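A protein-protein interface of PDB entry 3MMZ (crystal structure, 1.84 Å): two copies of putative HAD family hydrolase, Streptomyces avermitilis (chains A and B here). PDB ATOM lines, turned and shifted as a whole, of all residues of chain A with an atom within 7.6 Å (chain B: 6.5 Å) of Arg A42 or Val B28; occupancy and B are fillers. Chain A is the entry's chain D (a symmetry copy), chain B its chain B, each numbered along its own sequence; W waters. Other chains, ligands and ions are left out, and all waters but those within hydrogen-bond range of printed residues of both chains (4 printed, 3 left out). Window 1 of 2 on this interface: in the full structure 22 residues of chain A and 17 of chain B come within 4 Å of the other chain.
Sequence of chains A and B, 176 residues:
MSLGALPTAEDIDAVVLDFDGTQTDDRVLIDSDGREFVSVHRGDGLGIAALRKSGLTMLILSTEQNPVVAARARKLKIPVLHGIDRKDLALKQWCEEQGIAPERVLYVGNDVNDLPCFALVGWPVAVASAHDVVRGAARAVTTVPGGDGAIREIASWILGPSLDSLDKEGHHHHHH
The side-chain carboxylate of Asp B20 lies within salt-bridge range of the guanidinium group of Arg A42. The backbone carbonyl oxygen (O) of Asp B26 sits at hydrogen-bond distance from the backbone NH (N) of Arg A42 (2.8 Å). The backbone carbonyl oxygen of Val B28 is in hydrogen-bond range of the backbone NH of Val A40 (2.8 Å). N of Ile B30 is in hydrogen-bond range of O of Val A38 (2.9 Å). The guanidinium group (NH2) of Arg A42 lies within salt-bridge range of the side-chain carboxylate (OE1) of Glu B36, 2.6 Å away. OE2 of Glu B64 lies within salt-bridge range of NH1 of Arg A42, at 3.4 Å. The side-chain carboxylate of Glu B64 lies within salt-bridge range of the side-chain amino group of Lys A75, 2.7 Å away. The side-chain carboxylate (OD1) of Asp B111 is in salt-bridge range of the guanidinium group (NH1) of Arg A152 (2.8 Å).
N of Gly B21 is in hydrogen-bond range of OD1 of Asp B26. OD1 of Asp B25 sits at hydrogen-bond distance from N of Arg B27, at 3.0 Å. The backbone carbonyl oxygen of Phe B37 is in hydrogen-bond range of the backbone NH of Leu B29, at 2.8 Å. ND1 of His A41 sits at hydrogen-bond distance from N of Gly A43 (3.0 Å).
Phe A37 touches Leu B29. CA of Phe A37 touches O of Ile B30 (3.3 Å). O of Val A38 touches O of Val B28 (3.7 Å). Ser A39 touches Arg B27. Ser A39 touches Val B28. Ser A39 touches Leu B29 (OG to CD1, 3.5 Å). CA of His A41 touches O of Asp B26 (3.5 Å). Leu A46 touches Asp B111 (CD2 to OD2, 3.4 Å). Arg A72 touches Ile B30. Gly A147 touches Arg B27.
Printed residues of chain B within 4 Å of Ser A39: Arg B27, Val B28 and Leu B29. Printed residues of chain B within 4 Å of Val A40: Arg B27 (3.4 Å) and Val B28 (2.8 Å). Arg A42 touches five residues of chain B. Printed residues of chain B within 4 Å of Gly A147: Arg B27. Of the printed residues of chain A, Asp B20 touches Arg A42 (3.1 Å). Of chain A, only Val A38 (3.7 Å), Ser A39 (3.3 Å), Val A40 (2.8 Å) and Arg A42 (3.4 Å) come within 4 Å of Val B28.
Hydrophobic or aromatic side chains of chain A that line the printed part of chain B: Phe A37, Val A38, Val A40, His A41 and Leu A46. Printed residues of chain B that touch a printed residue of chain A: Asp B20, Asp B26, Arg B27, Val B28, Leu B29, Ile B30, Glu B36, Glu B64 and Asp B111. Hydrophobic or aromatic side chains of chain B that line the printed part of chain A: Val B28, Leu B29 and Ile B30. Along chain B the printed residues that touch a printed residue of chain A span positions 20 to 111. Among the printed residues, 22 pairs touch across the chains.
Positions printed for both chains: 37 and 38.
Water W4 bridges O of Ser A39 (2.6 Å) and NH1 of Arg B27 (3.5 Å). Water W2 lies within hydrogen-bond range of a ring nitrogen (NE2) of His A41 and the backbone carbonyl oxygen (O) of Asp B25. Water W1 bridges NH1 of Arg A72 (2.9 Å) and OE2 of Glu B36 (3.3 Å).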
ATOM      1  N   GLN A  23      -6.641   4.288 -29.424  1.00  0.00           N
ATOM      2  CA  GLN A  23      -7.659   3.384 -28.865  1.00  0.00           C
ATOM      3  C   GLN A  23      -7.884   3.668 -27.377  1.00  0.00           C
ATOM      4  O   GLN A  23      -8.725   3.034 -26.739  1.00  0.00           O
ATOM      5  CB  GLN A  23      -7.219   1.930 -29.047  1.00  0.00           C
ATOM      6  CG  GLN A  23      -7.067   1.532 -30.490  1.00  0.00           C
ATOM      7  CD  GLN A  23      -6.576   0.103 -30.657  1.00  0.00           C
ATOM      8  OE1 GLN A  23      -7.275  -0.853 -30.317  1.00  0.00           O
ATOM      9  NE2 GLN A  23      -5.358  -0.045 -31.160  1.00  0.00           N
ATOM     10  N   PHE A  37      -2.963  -0.122 -16.013  1.00  0.00           N
ATOM     11  CA  PHE A  37      -4.222  -0.473 -16.661  1.00  0.00           C
ATOM     12  C   PHE A  37      -4.537   0.644 -17.658  1.00  0.00           C
ATOM     13  O   PHE A  37      -4.125   1.789 -17.455  1.00  0.00           O
ATOM     14  CB  PHE A  37      -5.358  -0.587 -15.636  1.00  0.00           C
ATOM     15  CG  PHE A  37      -5.024  -1.445 -14.432  1.00  0.00           C
ATOM     16  CD1 PHE A  37      -4.160  -0.983 -13.438  1.00  0.00           C
ATOM     17  CD2 PHE A  37      -5.582  -2.707 -14.293  1.00  0.00           C
ATOM     18  CE1 PHE A  37      -3.840  -1.779 -12.321  1.00  0.00           C
ATOM     19  CE2 PHE A  37      -5.281  -3.516 -13.172  1.00  0.00           C
ATOM     20  CZ  PHE A  37      -4.406  -3.050 -12.194  1.00  0.00           C
ATOM     21  N   VAL A  38      -5.232   0.319 -18.745  1.00  0.00           N
ATOM     22  CA  VAL A  38      -5.708   1.352 -19.675  1.00  0.00           C
ATOM     23  C   VAL A  38      -7.183   1.127 -20.006  1.00  0.00           C
ATOM     24  O   VAL A  38      -7.680   0.008 -19.884  1.00  0.00           O
ATOM     25  CB  VAL A  38      -4.868   1.427 -20.990  1.00  0.00           C
ATOM     26  CG1 VAL A  38      -3.389   1.735 -20.686  1.00  0.00           C
ATOM     27  CG2 VAL A  38      -4.997   0.127 -21.796  1.00  0.00           C
ATOM     28  N   SER A  39      -7.884   2.190 -20.400  1.00  0.00           N
ATOM     29  CA  SER A  39      -9.286   2.046 -20.800  1.00  0.00           C
ATOM     30  C   SER A  39      -9.404   2.026 -22.310  1.00  0.00           C
ATOM     31  O   SER A  39      -8.901   2.920 -23.003  1.00  0.00           O
ATOM     32  CB  SER A  39     -10.171   3.153 -20.197  1.00  0.00           C
ATOM     33  OG  SER A  39     -10.148   3.074 -18.782  1.00  0.00           O
ATOM     34  N   VAL A  40     -10.059   0.991 -22.816  1.00  0.00           N
ATOM     35  CA  VAL A  40     -10.385   0.889 -24.227  1.00  0.00           C
ATOM     36  C   VAL A  40     -11.911   1.038 -24.370  1.00  0.00           C
ATOM     37  O   VAL A  40     -12.609   1.246 -23.374  1.00  0.00           O
ATOM     38  CB  VAL A  40      -9.843  -0.424 -24.863  1.00  0.00           C
ATOM     39  CG1 VAL A  40      -8.299  -0.401 -24.902  1.00  0.00           C
ATOM     40  CG2 VAL A  40     -10.370  -1.675 -24.128  1.00  0.00           C
ATOM     41  N   HIS A  41     -12.423   0.923 -25.592  1.00  0.00           N
ATOM     42  CA  HIS A  41     -13.836   1.235 -25.860  1.00  0.00           C
ATOM     43  C   HIS A  41     -14.513   0.099 -26.629  1.00  0.00           C
ATOM     44  O   HIS A  41     -13.968  -0.387 -27.615  1.00  0.00           O
ATOM     45  CB  HIS A  41     -13.886   2.550 -26.652  1.00  0.00           C
ATOM     46  CG  HIS A  41     -15.239   3.186 -26.724  1.00  0.00           C
ATOM     47  ND1 HIS A  41     -16.163   2.860 -27.695  1.00  0.00           N
ATOM     48  CD2 HIS A  41     -15.806   4.162 -25.976  1.00  0.00           C
ATOM     49  CE1 HIS A  41     -17.250   3.592 -27.528  1.00  0.00           C
ATOM     50  NE2 HIS A  41     -17.061   4.389 -26.491  1.00  0.00           N
ATOM     51  N   ARG A  42     -15.700  -0.312 -26.170  1.00  0.00           N
ATOM     52  CA  ARG A  42     -16.429  -1.443 -26.769  1.00  0.00           C
ATOM     53  C   ARG A  42     -16.934  -1.136 -28.167  1.00  0.00           C
ATOM     54  O   ARG A  42     -17.059  -2.036 -28.996  1.00  0.00           O
ATOM     55  CB  ARG A  42     -17.606  -1.879 -25.891  1.00  0.00           C
ATOM     56  CG  ARG A  42     -17.203  -2.584 -24.600  1.00  0.00           C
ATOM     57  CD  ARG A  42     -17.068  -4.103 -24.788  1.00  0.00           C
ATOM     58  NE  ARG A  42     -16.909  -4.781 -23.504  1.00  0.00           N
ATOM     59  CZ  ARG A  42     -15.855  -5.512 -23.148  1.00  0.00           C
ATOM     60  NH1 ARG A  42     -14.842  -5.696 -23.981  1.00  0.00           N
ATOM     61  NH2 ARG A  42     -15.829  -6.072 -21.946  1.00  0.00           N
ATOM     62  N   GLY A  43     -17.261   0.130 -28.406  1.00  0.00           N
ATOM     63  CA  GLY A  43     -17.594   0.607 -29.748  1.00  0.00           C
ATOM     64  C   GLY A  43     -16.440   0.410 -30.717  1.00  0.00           C
ATOM     65  O   GLY A  43     -16.645  -0.086 -31.831  1.00  0.00           O
ATOM     66  N   ASP A  44     -15.225   0.794 -30.312  1.00  0.00           N
ATOM     67  CA  ASP A  44     -14.026   0.503 -31.110  1.00  0.00           C
ATOM     68  C   ASP A  44     -13.924  -0.994 -31.403  1.00  0.00           C
ATOM     69  O   ASP A  44     -13.607  -1.399 -32.522  1.00  0.00           O
ATOM     70  CB  ASP A  44     -12.739   0.947 -30.391  1.00  0.00           C
ATOM     71  CG  ASP A  44     -12.561   2.458 -30.351  1.00  0.00           C
ATOM     72  OD1 ASP A  44     -13.178   3.182 -31.163  1.00  0.00           O
ATOM     73  OD2 ASP A  44     -11.771   2.922 -29.499  1.00  0.00           O
ATOM     74  N   GLY A  45     -14.169  -1.813 -30.384  1.00  0.00           N
ATOM     75  CA  GLY A  45     -14.107  -3.260 -30.524  1.00  0.00           C
ATOM     76  C   GLY A  45     -15.065  -3.781 -31.580  1.00  0.00           C
ATOM     77  O   GLY A  45     -14.715  -4.647 -32.374  1.00  0.00           O
ATOM     78  N   LEU A  46     -16.271  -3.224 -31.605  1.00  0.00           N
ATOM     79  CA  LEU A  46     -17.281  -3.642 -32.571  1.00  0.00           C
ATOM     80  C   LEU A  46     -16.901  -3.168 -33.959  1.00  0.00           C
ATOM     81  O   LEU A  46     -17.087  -3.903 -34.930  1.00  0.00           O
ATOM     82  CB  LEU A  46     -18.672  -3.119 -32.166  1.00  0.00           C
ATOM     83  CG  LEU A  46     -19.864  -3.566 -33.017  1.00  0.00           C
ATOM     84  CD1 LEU A  46     -20.252  -5.013 -32.723  1.00  0.00           C
ATOM     85  CD2 LEU A  46     -21.054  -2.637 -32.781  1.00  0.00           C
ATOM     86  N   GLY A  47     -16.368  -1.947 -34.044  1.00  0.00           N
ATOM     87  CA  GLY A  47     -15.884  -1.377 -35.305  1.00  0.00           C
ATOM     88  C   GLY A  47     -14.739  -2.191 -35.893  1.00  0.00           C
ATOM     89  O   GLY A  47     -14.731  -2.505 -37.075  1.00  0.00           O
ATOM     90  N   ILE A  48     -13.757  -2.505 -35.059  1.00  0.00           N
ATOM     91  CA  ILE A  48     -12.605  -3.309 -35.471  1.00  0.00           C
ATOM     92  C   ILE A  48     -13.044  -4.695 -35.968  1.00  0.00           C
ATOM     93  O   ILE A  48     -12.580  -5.165 -37.015  1.00  0.00           O
ATOM     94  CB  ILE A  48     -11.577  -3.398 -34.314  1.00  0.00           C
ATOM     95  CG1 ILE A  48     -10.927  -2.023 -34.101  1.00  0.00           C
ATOM     96  CG2 ILE A  48     -10.529  -4.487 -34.575  1.00  0.00           C
ATOM     97  CD1 ILE A  48     -10.229  -1.815 -32.738  1.00  0.00           C
ATOM     98  N   ARG A  72      -5.025  -6.527 -25.596  1.00  0.00           N
ATOM     99  CA  ARG A  72      -6.118  -5.955 -26.386  1.00  0.00           C
ATOM    100  C   ARG A  72      -6.169  -6.600 -27.770  1.00  0.00           C
ATOM    101  O   ARG A  72      -7.239  -6.987 -28.248  1.00  0.00           O
ATOM    102  CB  ARG A  72      -5.950  -4.438 -26.526  1.00  0.00           C
ATOM    103  CG  ARG A  72      -7.075  -3.753 -27.293  1.00  0.00           C
ATOM    104  CD  ARG A  72      -8.428  -4.031 -26.631  1.00  0.00           C
ATOM    105  NE  ARG A  72      -9.496  -3.247 -27.242  1.00  0.00           N
ATOM    106  CZ  ARG A  72     -10.791  -3.519 -27.129  1.00  0.00           C
ATOM    107  NH1 ARG A  72     -11.214  -4.546 -26.395  1.00  0.00           N
ATOM    108  NH2 ARG A  72     -11.661  -2.741 -27.747  1.00  0.00           N
ATOM    109  N   LYS A  75      -7.735 -10.100 -27.610  1.00  0.00           N
ATOM    110  CA  LYS A  75      -9.188 -10.054 -27.503  1.00  0.00           C
ATOM    111  C   LYS A  75      -9.845  -9.675 -28.837  1.00  0.00           C
ATOM    112  O   LYS A  75     -10.889 -10.219 -29.189  1.00  0.00           O
ATOM    113  CB  LYS A  75      -9.610  -9.141 -26.332  1.00  0.00           C
ATOM    114  CG  LYS A  75     -10.515  -7.955 -26.671  1.00  0.00           C
ATOM    115  CD  LYS A  75     -11.974  -8.326 -26.894  1.00  0.00           C
ATOM    116  CE  LYS A  75     -12.763  -8.417 -25.606  1.00  0.00           C
ATOM    117  NZ  LYS A  75     -14.200  -8.539 -25.935  1.00  0.00           N
ATOM    118  N   LEU A  76      -9.216  -8.765 -29.577  1.00  0.00           N
ATOM    119  CA  LEU A  76      -9.727  -8.325 -30.874  1.00  0.00           C
ATOM    120  C   LEU A  76      -9.415  -9.307 -32.019  1.00  0.00           C
ATOM    121  O   LEU A  76      -9.913  -9.134 -33.132  1.00  0.00           O
ATOM    122  CB  LEU A  76      -9.169  -6.936 -31.220  1.00  0.00           C
ATOM    123  CG  LEU A  76      -9.547  -5.753 -30.322  1.00  0.00           C
ATOM    124  CD1 LEU A  76      -8.782  -4.506 -30.756  1.00  0.00           C
ATOM    125  CD2 LEU A  76     -11.049  -5.511 -30.336  1.00  0.00           C
ATOM    126  N   GLY A 147     -10.117   6.793 -27.276  1.00  0.00           N
ATOM    127  CA  GLY A 147     -10.701   6.150 -26.099  1.00  0.00           C
ATOM    128  C   GLY A 147     -12.202   6.335 -25.980  1.00  0.00           C
ATOM    129  O   GLY A 147     -12.840   5.730 -25.101  1.00  0.00           O
ATOM    130  N   ASP A 148     -12.764   7.166 -26.858  1.00  0.00           N
ATOM    131  CA  ASP A 148     -14.186   7.507 -26.826  1.00  0.00           C
ATOM    132  C   ASP A 148     -14.949   6.885 -28.011  1.00  0.00           C
ATOM    133  O   ASP A 148     -16.148   7.133 -28.184  1.00  0.00           O
ATOM    134  CB  ASP A 148     -14.335   9.039 -26.801  1.00  0.00           C
ATOM    135  CG  ASP A 148     -15.731   9.504 -26.409  1.00  0.00           C
ATOM    136  OD1 ASP A 148     -16.434   8.783 -25.672  1.00  0.00           O
ATOM    137  OD2 ASP A 148     -16.119  10.616 -26.833  1.00  0.00           O
ATOM    138  N   GLY A 149     -14.259   6.075 -28.821  1.00  0.00           N
ATOM    139  CA  GLY A 149     -14.872   5.420 -29.991  1.00  0.00           C
ATOM    140  C   GLY A 149     -14.469   5.986 -31.343  1.00  0.00           C
ATOM    141  O   GLY A 149     -15.248   5.957 -32.296  1.00  0.00           O
ATOM    142  N   ARG A 152     -14.495   3.224 -33.954  1.00  0.00           N
ATOM    143  CA  ARG A 152     -15.871   2.960 -34.345  1.00  0.00           C
ATOM    144  C   ARG A 152     -16.368   3.976 -35.374  1.00  0.00           C
ATOM    145  O   ARG A 152     -17.035   3.605 -36.333  1.00  0.00           O
ATOM    146  CB  ARG A 152     -16.821   2.908 -33.151  1.00  0.00           C
ATOM    147  CG  ARG A 152     -18.119   2.173 -33.520  1.00  0.00           C
ATOM    148  CD  ARG A 152     -19.286   2.745 -32.818  1.00  0.00           C
ATOM    149  NE  ARG A 152     -20.580   2.251 -33.333  1.00  0.00           N
ATOM    150  CZ  ARG A 152     -21.192   2.721 -34.420  1.00  0.00           C
ATOM    151  NH1 ARG A 152     -22.370   2.239 -34.788  1.00  0.00           N
ATOM    152  NH2 ARG A 152     -20.621   3.675 -35.158  1.00  0.00           N
ATOM    153  N   PHE B  19     -25.754  -4.742 -21.998  1.00  0.00           N
ATOM    154  CA  PHE B  19     -24.831  -4.377 -20.927  1.00  0.00           C
ATOM    155  C   PHE B  19     -23.898  -3.207 -21.291  1.00  0.00           C
ATOM    156  O   PHE B  19     -24.185  -2.058 -20.941  1.00  0.00           O
ATOM    157  CB  PHE B  19     -24.037  -5.598 -20.449  1.00  0.00           C
ATOM    158  CG  PHE B  19     -23.196  -5.318 -19.248  1.00  0.00           C
ATOM    159  CD1 PHE B  19     -23.788  -4.956 -18.046  1.00  0.00           C
ATOM    160  CD2 PHE B  19     -21.814  -5.365 -19.332  1.00  0.00           C
ATOM    161  CE1 PHE B  19     -23.017  -4.682 -16.929  1.00  0.00           C
ATOM    162  CE2 PHE B  19     -21.034  -5.091 -18.223  1.00  0.00           C
ATOM    163  CZ  PHE B  19     -21.639  -4.741 -17.021  1.00  0.00           C
ATOM    164  N   ASP B  20     -22.801  -3.484 -21.996  1.00  0.00           N
ATOM    165  CA  ASP B  20     -21.802  -2.429 -22.304  1.00  0.00           C
ATOM    166  C   ASP B  20     -22.439  -1.289 -23.097  1.00  0.00           C
ATOM    167  O   ASP B  20     -23.110  -1.538 -24.096  1.00  0.00           O
ATOM    168  CB  ASP B  20     -20.625  -2.998 -23.103  1.00  0.00           C
ATOM    169  CG  ASP B  20     -19.819  -4.032 -22.321  1.00  0.00           C
ATOM    170  OD1 ASP B  20     -19.098  -3.664 -21.373  1.00  0.00           O
ATOM    171  OD2 ASP B  20     -19.899  -5.224 -22.672  1.00  0.00           O
ATOM    172  N   GLY B  21     -22.256  -0.047 -22.645  1.00  0.00           N
ATOM    173  CA  GLY B  21     -22.809   1.102 -23.364  1.00  0.00           C
ATOM    174  C   GLY B  21     -24.256   1.435 -23.040  1.00  0.00           C
ATOM    175  O   GLY B  21     -24.748   2.512 -23.391  1.00  0.00           O
ATOM    176  N   THR B  24     -23.306   0.821 -18.969  1.00  0.00           N
ATOM    177  CA  THR B  24     -21.983   1.423 -18.811  1.00  0.00           C
ATOM    178  C   THR B  24     -21.816   2.485 -19.898  1.00  0.00           C
ATOM    179  O   THR B  24     -22.642   2.598 -20.806  1.00  0.00           O
ATOM    180  CB  THR B  24     -20.816   0.402 -18.989  1.00  0.00           C
ATOM    181  OG1 THR B  24     -20.615   0.145 -20.381  1.00  0.00           O
ATOM    182  CG2 THR B  24     -21.068  -0.935 -18.261  1.00  0.00           C
ATOM    183  N   ASP B  25     -20.716   3.227 -19.819  1.00  0.00           N
ATOM    184  CA  ASP B  25     -20.384   4.210 -20.840  1.00  0.00           C
ATOM    185  C   ASP B  25     -19.558   3.633 -22.000  1.00  0.00           C
ATOM    186  O   ASP B  25     -18.933   4.396 -22.762  1.00  0.00           O
ATOM    187  CB  ASP B  25     -19.639   5.379 -20.196  1.00  0.00           C
ATOM    188  CG  ASP B  25     -18.308   4.967 -19.605  1.00  0.00           C
ATOM    189  OD1 ASP B  25     -17.913   3.787 -19.756  1.00  0.00           O
ATOM    190  OD2 ASP B  25     -17.650   5.829 -18.977  1.00  0.00           O
ATOM    191  N   ASP B  26     -19.556   2.300 -22.123  1.00  0.00           N
ATOM    192  CA  ASP B  26     -18.867   1.575 -23.210  1.00  0.00           C
ATOM    193  C   ASP B  26     -17.350   1.500 -23.023  1.00  0.00           C
ATOM    194  O   ASP B  26     -16.653   0.927 -23.864  1.00  0.00           O
ATOM    195  CB  ASP B  26     -19.195   2.167 -24.594  1.00  0.00           C
ATOM    196  CG  ASP B  26     -20.045   1.253 -25.463  1.00  0.00           C
ATOM    197  OD1 ASP B  26     -20.249   0.057 -25.144  1.00  0.00           O
ATOM    198  OD2 ASP B  26     -20.512   1.752 -26.510  1.00  0.00           O
ATOM    199  N   ARG B  27     -16.834   2.072 -21.935  1.00  0.00           N
ATOM    200  CA  ARG B  27     -15.408   1.952 -21.628  1.00  0.00           C
ATOM    201  C   ARG B  27     -15.118   0.657 -20.871  1.00  0.00           C
ATOM    202  O   ARG B  27     -15.964   0.142 -20.127  1.00  0.00           O
ATOM    203  CB  ARG B  27     -14.892   3.170 -20.851  1.00  0.00           C
ATOM    204  CG  ARG B  27     -14.932   4.479 -21.643  1.00  0.00           C
ATOM    205  CD  ARG B  27     -14.480   5.663 -20.790  1.00  0.00           C
ATOM    206  NE  ARG B  27     -13.942   6.758 -21.601  1.00  0.00           N
ATOM    207  CZ  ARG B  27     -12.696   7.231 -21.511  1.00  0.00           C
ATOM    208  NH1 ARG B  27     -11.838   6.718 -20.626  1.00  0.00           N
ATOM    209  NH2 ARG B  27     -12.307   8.228 -22.301  1.00  0.00           N
ATOM    210  N   VAL B  28     -13.922   0.113 -21.089  1.00  0.00           N
ATOM    211  CA  VAL B  28     -13.490  -1.098 -20.413  1.00  0.00           C
ATOM    212  C   VAL B  28     -12.050  -0.907 -19.970  1.00  0.00           C
ATOM    213  O   VAL B  28     -11.192  -0.618 -20.795  1.00  0.00           O
ATOM    214  CB  VAL B  28     -13.546  -2.332 -21.351  1.00  0.00           C
ATOM    215  CG1 VAL B  28     -13.244  -3.608 -20.570  1.00  0.00           C
ATOM    216  CG2 VAL B  28     -14.886  -2.434 -22.028  1.00  0.00           C
ATOM    217  N   LEU B  29     -11.790  -1.067 -18.674  1.00  0.00           N
ATOM    218  CA  LEU B  29     -10.423  -1.032 -18.172  1.00  0.00           C
ATOM    219  C   LEU B  29      -9.826  -2.427 -18.317  1.00  0.00           C
ATOM    220  O   LEU B  29     -10.476  -3.415 -17.969  1.00  0.00           O
ATOM    221  CB  LEU B  29     -10.389  -0.613 -16.702  1.00  0.00           C
ATOM    222  CG  LEU B  29      -9.023  -0.308 -16.072  1.00  0.00           C
ATOM    223  CD1 LEU B  29      -8.461   1.053 -16.537  1.00  0.00           C
ATOM    224  CD2 LEU B  29      -9.111  -0.348 -14.547  1.00  0.00           C
ATOM    225  N   ILE B  30      -8.597  -2.502 -18.815  1.00  0.00           N
ATOM    226  CA  ILE B  30      -7.952  -3.794 -19.041  1.00  0.00           C
ATOM    227  C   ILE B  30      -6.556  -3.840 -18.433  1.00  0.00           C
ATOM    228  O   ILE B  30      -5.880  -2.815 -18.350  1.00  0.00           O
ATOM    229  CB  ILE B  30      -7.918  -4.173 -20.549  1.00  0.00           C
ATOM    230  CG1 ILE B  30      -7.048  -3.190 -21.351  1.00  0.00           C
ATOM    231  CG2 ILE B  30      -9.365  -4.276 -21.125  1.00  0.00           C
ATOM    232  CD1 ILE B  30      -6.854  -3.584 -22.832  1.00  0.00           C
ATOM    233  N   ARG B  35      -7.883  -9.342 -17.757  1.00  0.00           N
ATOM    234  CA  ARG B  35      -8.943  -8.991 -16.812  1.00  0.00           C
ATOM    235  C   ARG B  35      -9.586  -7.688 -17.297  1.00  0.00           C
ATOM    236  O   ARG B  35      -8.888  -6.793 -17.778  1.00  0.00           O
ATOM    237  CB  ARG B  35      -8.356  -8.822 -15.404  1.00  0.00           C
ATOM    238  CG  ARG B  35      -9.331  -8.391 -14.302  1.00  0.00           C
ATOM    239  CD  ARG B  35     -10.035  -9.570 -13.613  1.00  0.00           C
ATOM    240  NE  ARG B  35      -9.113 -10.513 -12.969  1.00  0.00           N
ATOM    241  CZ  ARG B  35      -9.475 -11.447 -12.087  1.00  0.00           C
ATOM    242  NH1 ARG B  35     -10.746 -11.574 -11.717  1.00  0.00           N
ATOM    243  NH2 ARG B  35      -8.559 -12.252 -11.561  1.00  0.00           N
ATOM    244  N   GLU B  36     -10.913  -7.622 -17.208  1.00  0.00           N
ATOM    245  CA  GLU B  36     -11.674  -6.434 -17.592  1.00  0.00           C
ATOM    246  C   GLU B  36     -12.417  -5.836 -16.401  1.00  0.00           C
ATOM    247  O   GLU B  36     -12.822  -6.554 -15.479  1.00  0.00           O
ATOM    248  CB  GLU B  36     -12.647  -6.751 -18.741  1.00  0.00           C
ATOM    249  CG  GLU B  36     -11.966  -7.133 -20.080  1.00  0.00           C
ATOM    250  CD  GLU B  36     -12.959  -7.439 -21.207  1.00  0.00           C
ATOM    251  OE1 GLU B  36     -14.141  -7.689 -20.923  1.00  0.00           O
ATOM    252  OE2 GLU B  36     -12.557  -7.427 -22.390  1.00  0.00           O
ATOM    253  N   PHE B  37     -12.562  -4.513 -16.411  1.00  0.00           N
ATOM    254  CA  PHE B  37     -13.347  -3.810 -15.415  1.00  0.00           C
ATOM    255  C   PHE B  37     -14.251  -2.834 -16.149  1.00  0.00           C
ATOM    256  O   PHE B  37     -13.831  -2.183 -17.113  1.00  0.00           O
ATOM    257  CB  PHE B  37     -12.489  -2.953 -14.472  1.00  0.00           C
ATOM    258  CG  PHE B  37     -11.306  -3.648 -13.876  1.00  0.00           C
ATOM    259  CD1 PHE B  37     -10.277  -4.135 -14.679  1.00  0.00           C
ATOM    260  CD2 PHE B  37     -11.175  -3.732 -12.493  1.00  0.00           C
ATOM    261  CE1 PHE B  37      -9.163  -4.746 -14.127  1.00  0.00           C
ATOM    262  CE2 PHE B  37     -10.058  -4.344 -11.922  1.00  0.00           C
ATOM    263  CZ  PHE B  37      -9.053  -4.859 -12.747  1.00  0.00           C
ATOM    264  N   VAL B  38     -15.478  -2.698 -15.672  1.00  0.00           N
ATOM    265  CA  VAL B  38     -16.379  -1.691 -16.220  1.00  0.00           C
ATOM    266  C   VAL B  38     -17.031  -0.912 -15.082  1.00  0.00           C
ATOM    267  O   VAL B  38     -17.094  -1.405 -13.946  1.00  0.00           O
ATOM    268  CB  VAL B  38     -17.456  -2.302 -17.154  1.00  0.00           C
ATOM    269  CG1 VAL B  38     -16.797  -3.093 -18.299  1.00  0.00           C
ATOM    270  CG2 VAL B  38     -18.427  -3.195 -16.358  1.00  0.00           C
ATOM    271  N   GLU B  64     -20.753 -10.261 -25.332  1.00  0.00           N
ATOM    272  CA  GLU B  64     -19.439 -10.250 -24.683  1.00  0.00           C
ATOM    273  C   GLU B  64     -19.184 -11.518 -23.859  1.00  0.00           C
ATOM    274  O   GLU B  64     -19.987 -11.897 -23.005  1.00  0.00           O
ATOM    275  CB  GLU B  64     -19.283  -8.984 -23.819  1.00  0.00           C
ATOM    276  CG  GLU B  64     -17.949  -8.868 -23.088  1.00  0.00           C
ATOM    277  CD  GLU B  64     -16.750  -9.004 -24.013  1.00  0.00           C
ATOM    278  OE1 GLU B  64     -15.824  -9.776 -23.668  1.00  0.00           O
ATOM    279  OE2 GLU B  64     -16.739  -8.343 -25.083  1.00  0.00           O
ATOM    280  N   ASN B  66     -16.471 -12.001 -21.793  1.00  0.00           N
ATOM    281  CA  ASN B  66     -15.847 -11.759 -20.490  1.00  0.00           C
ATOM    282  C   ASN B  66     -16.855 -11.859 -19.336  1.00  0.00           C
ATOM    283  O   ASN B  66     -17.969 -11.349 -19.453  1.00  0.00           O
ATOM    284  CB  ASN B  66     -15.105 -10.423 -20.444  1.00  0.00           C
ATOM    285  CG  ASN B  66     -14.275 -10.269 -19.186  1.00  0.00           C
ATOM    286  OD1 ASN B  66     -14.801  -9.946 -18.121  1.00  0.00           O
ATOM    287  ND2 ASN B  66     -12.973 -10.509 -19.299  1.00  0.00           N
ATOM    288  N   VAL B  68     -17.245 -10.337 -16.611  1.00  0.00           N
ATOM    289  CA  VAL B  68     -17.627  -9.121 -15.878  1.00  0.00           C
ATOM    290  C   VAL B  68     -19.148  -8.845 -15.973  1.00  0.00           C
ATOM    291  O   VAL B  68     -19.776  -8.454 -14.986  1.00  0.00           O
ATOM    292  CB  VAL B  68     -16.737  -7.899 -16.271  1.00  0.00           C
ATOM    293  CG1 VAL B  68     -16.899  -7.552 -17.736  1.00  0.00           C
ATOM    294  CG2 VAL B  68     -17.023  -6.698 -15.379  1.00  0.00           C
ATOM    295  N   ASP B 111     -26.114   0.198 -29.569  1.00  0.00           N
ATOM    296  CA  ASP B 111     -25.294   0.086 -30.794  1.00  0.00           C
ATOM    297  C   ASP B 111     -25.935  -0.834 -31.840  1.00  0.00           C
ATOM    298  O   ASP B 111     -26.997  -1.424 -31.603  1.00  0.00           O
ATOM    299  CB  ASP B 111     -23.841  -0.340 -30.475  1.00  0.00           C
ATOM    300  CG  ASP B 111     -22.796   0.257 -31.468  1.00  0.00           C
ATOM    301  OD1 ASP B 111     -23.143   0.656 -32.598  1.00  0.00           O
ATOM    302  OD2 ASP B 111     -21.599   0.329 -31.117  1.00  0.00           O
HETATM  303  O   HOH W   1     -10.099  -6.079 -24.203  1.00  0.00           O
HETATM  304  O   HOH W   2     -19.005   6.255 -25.708  1.00  0.00           O
HETATM  305  O   HOH W   3     -18.164  -6.057 -20.273  1.00  0.00           O
HETATM  306  O   HOH W   4      -9.253   5.439 -22.550  1.00  0.00           O
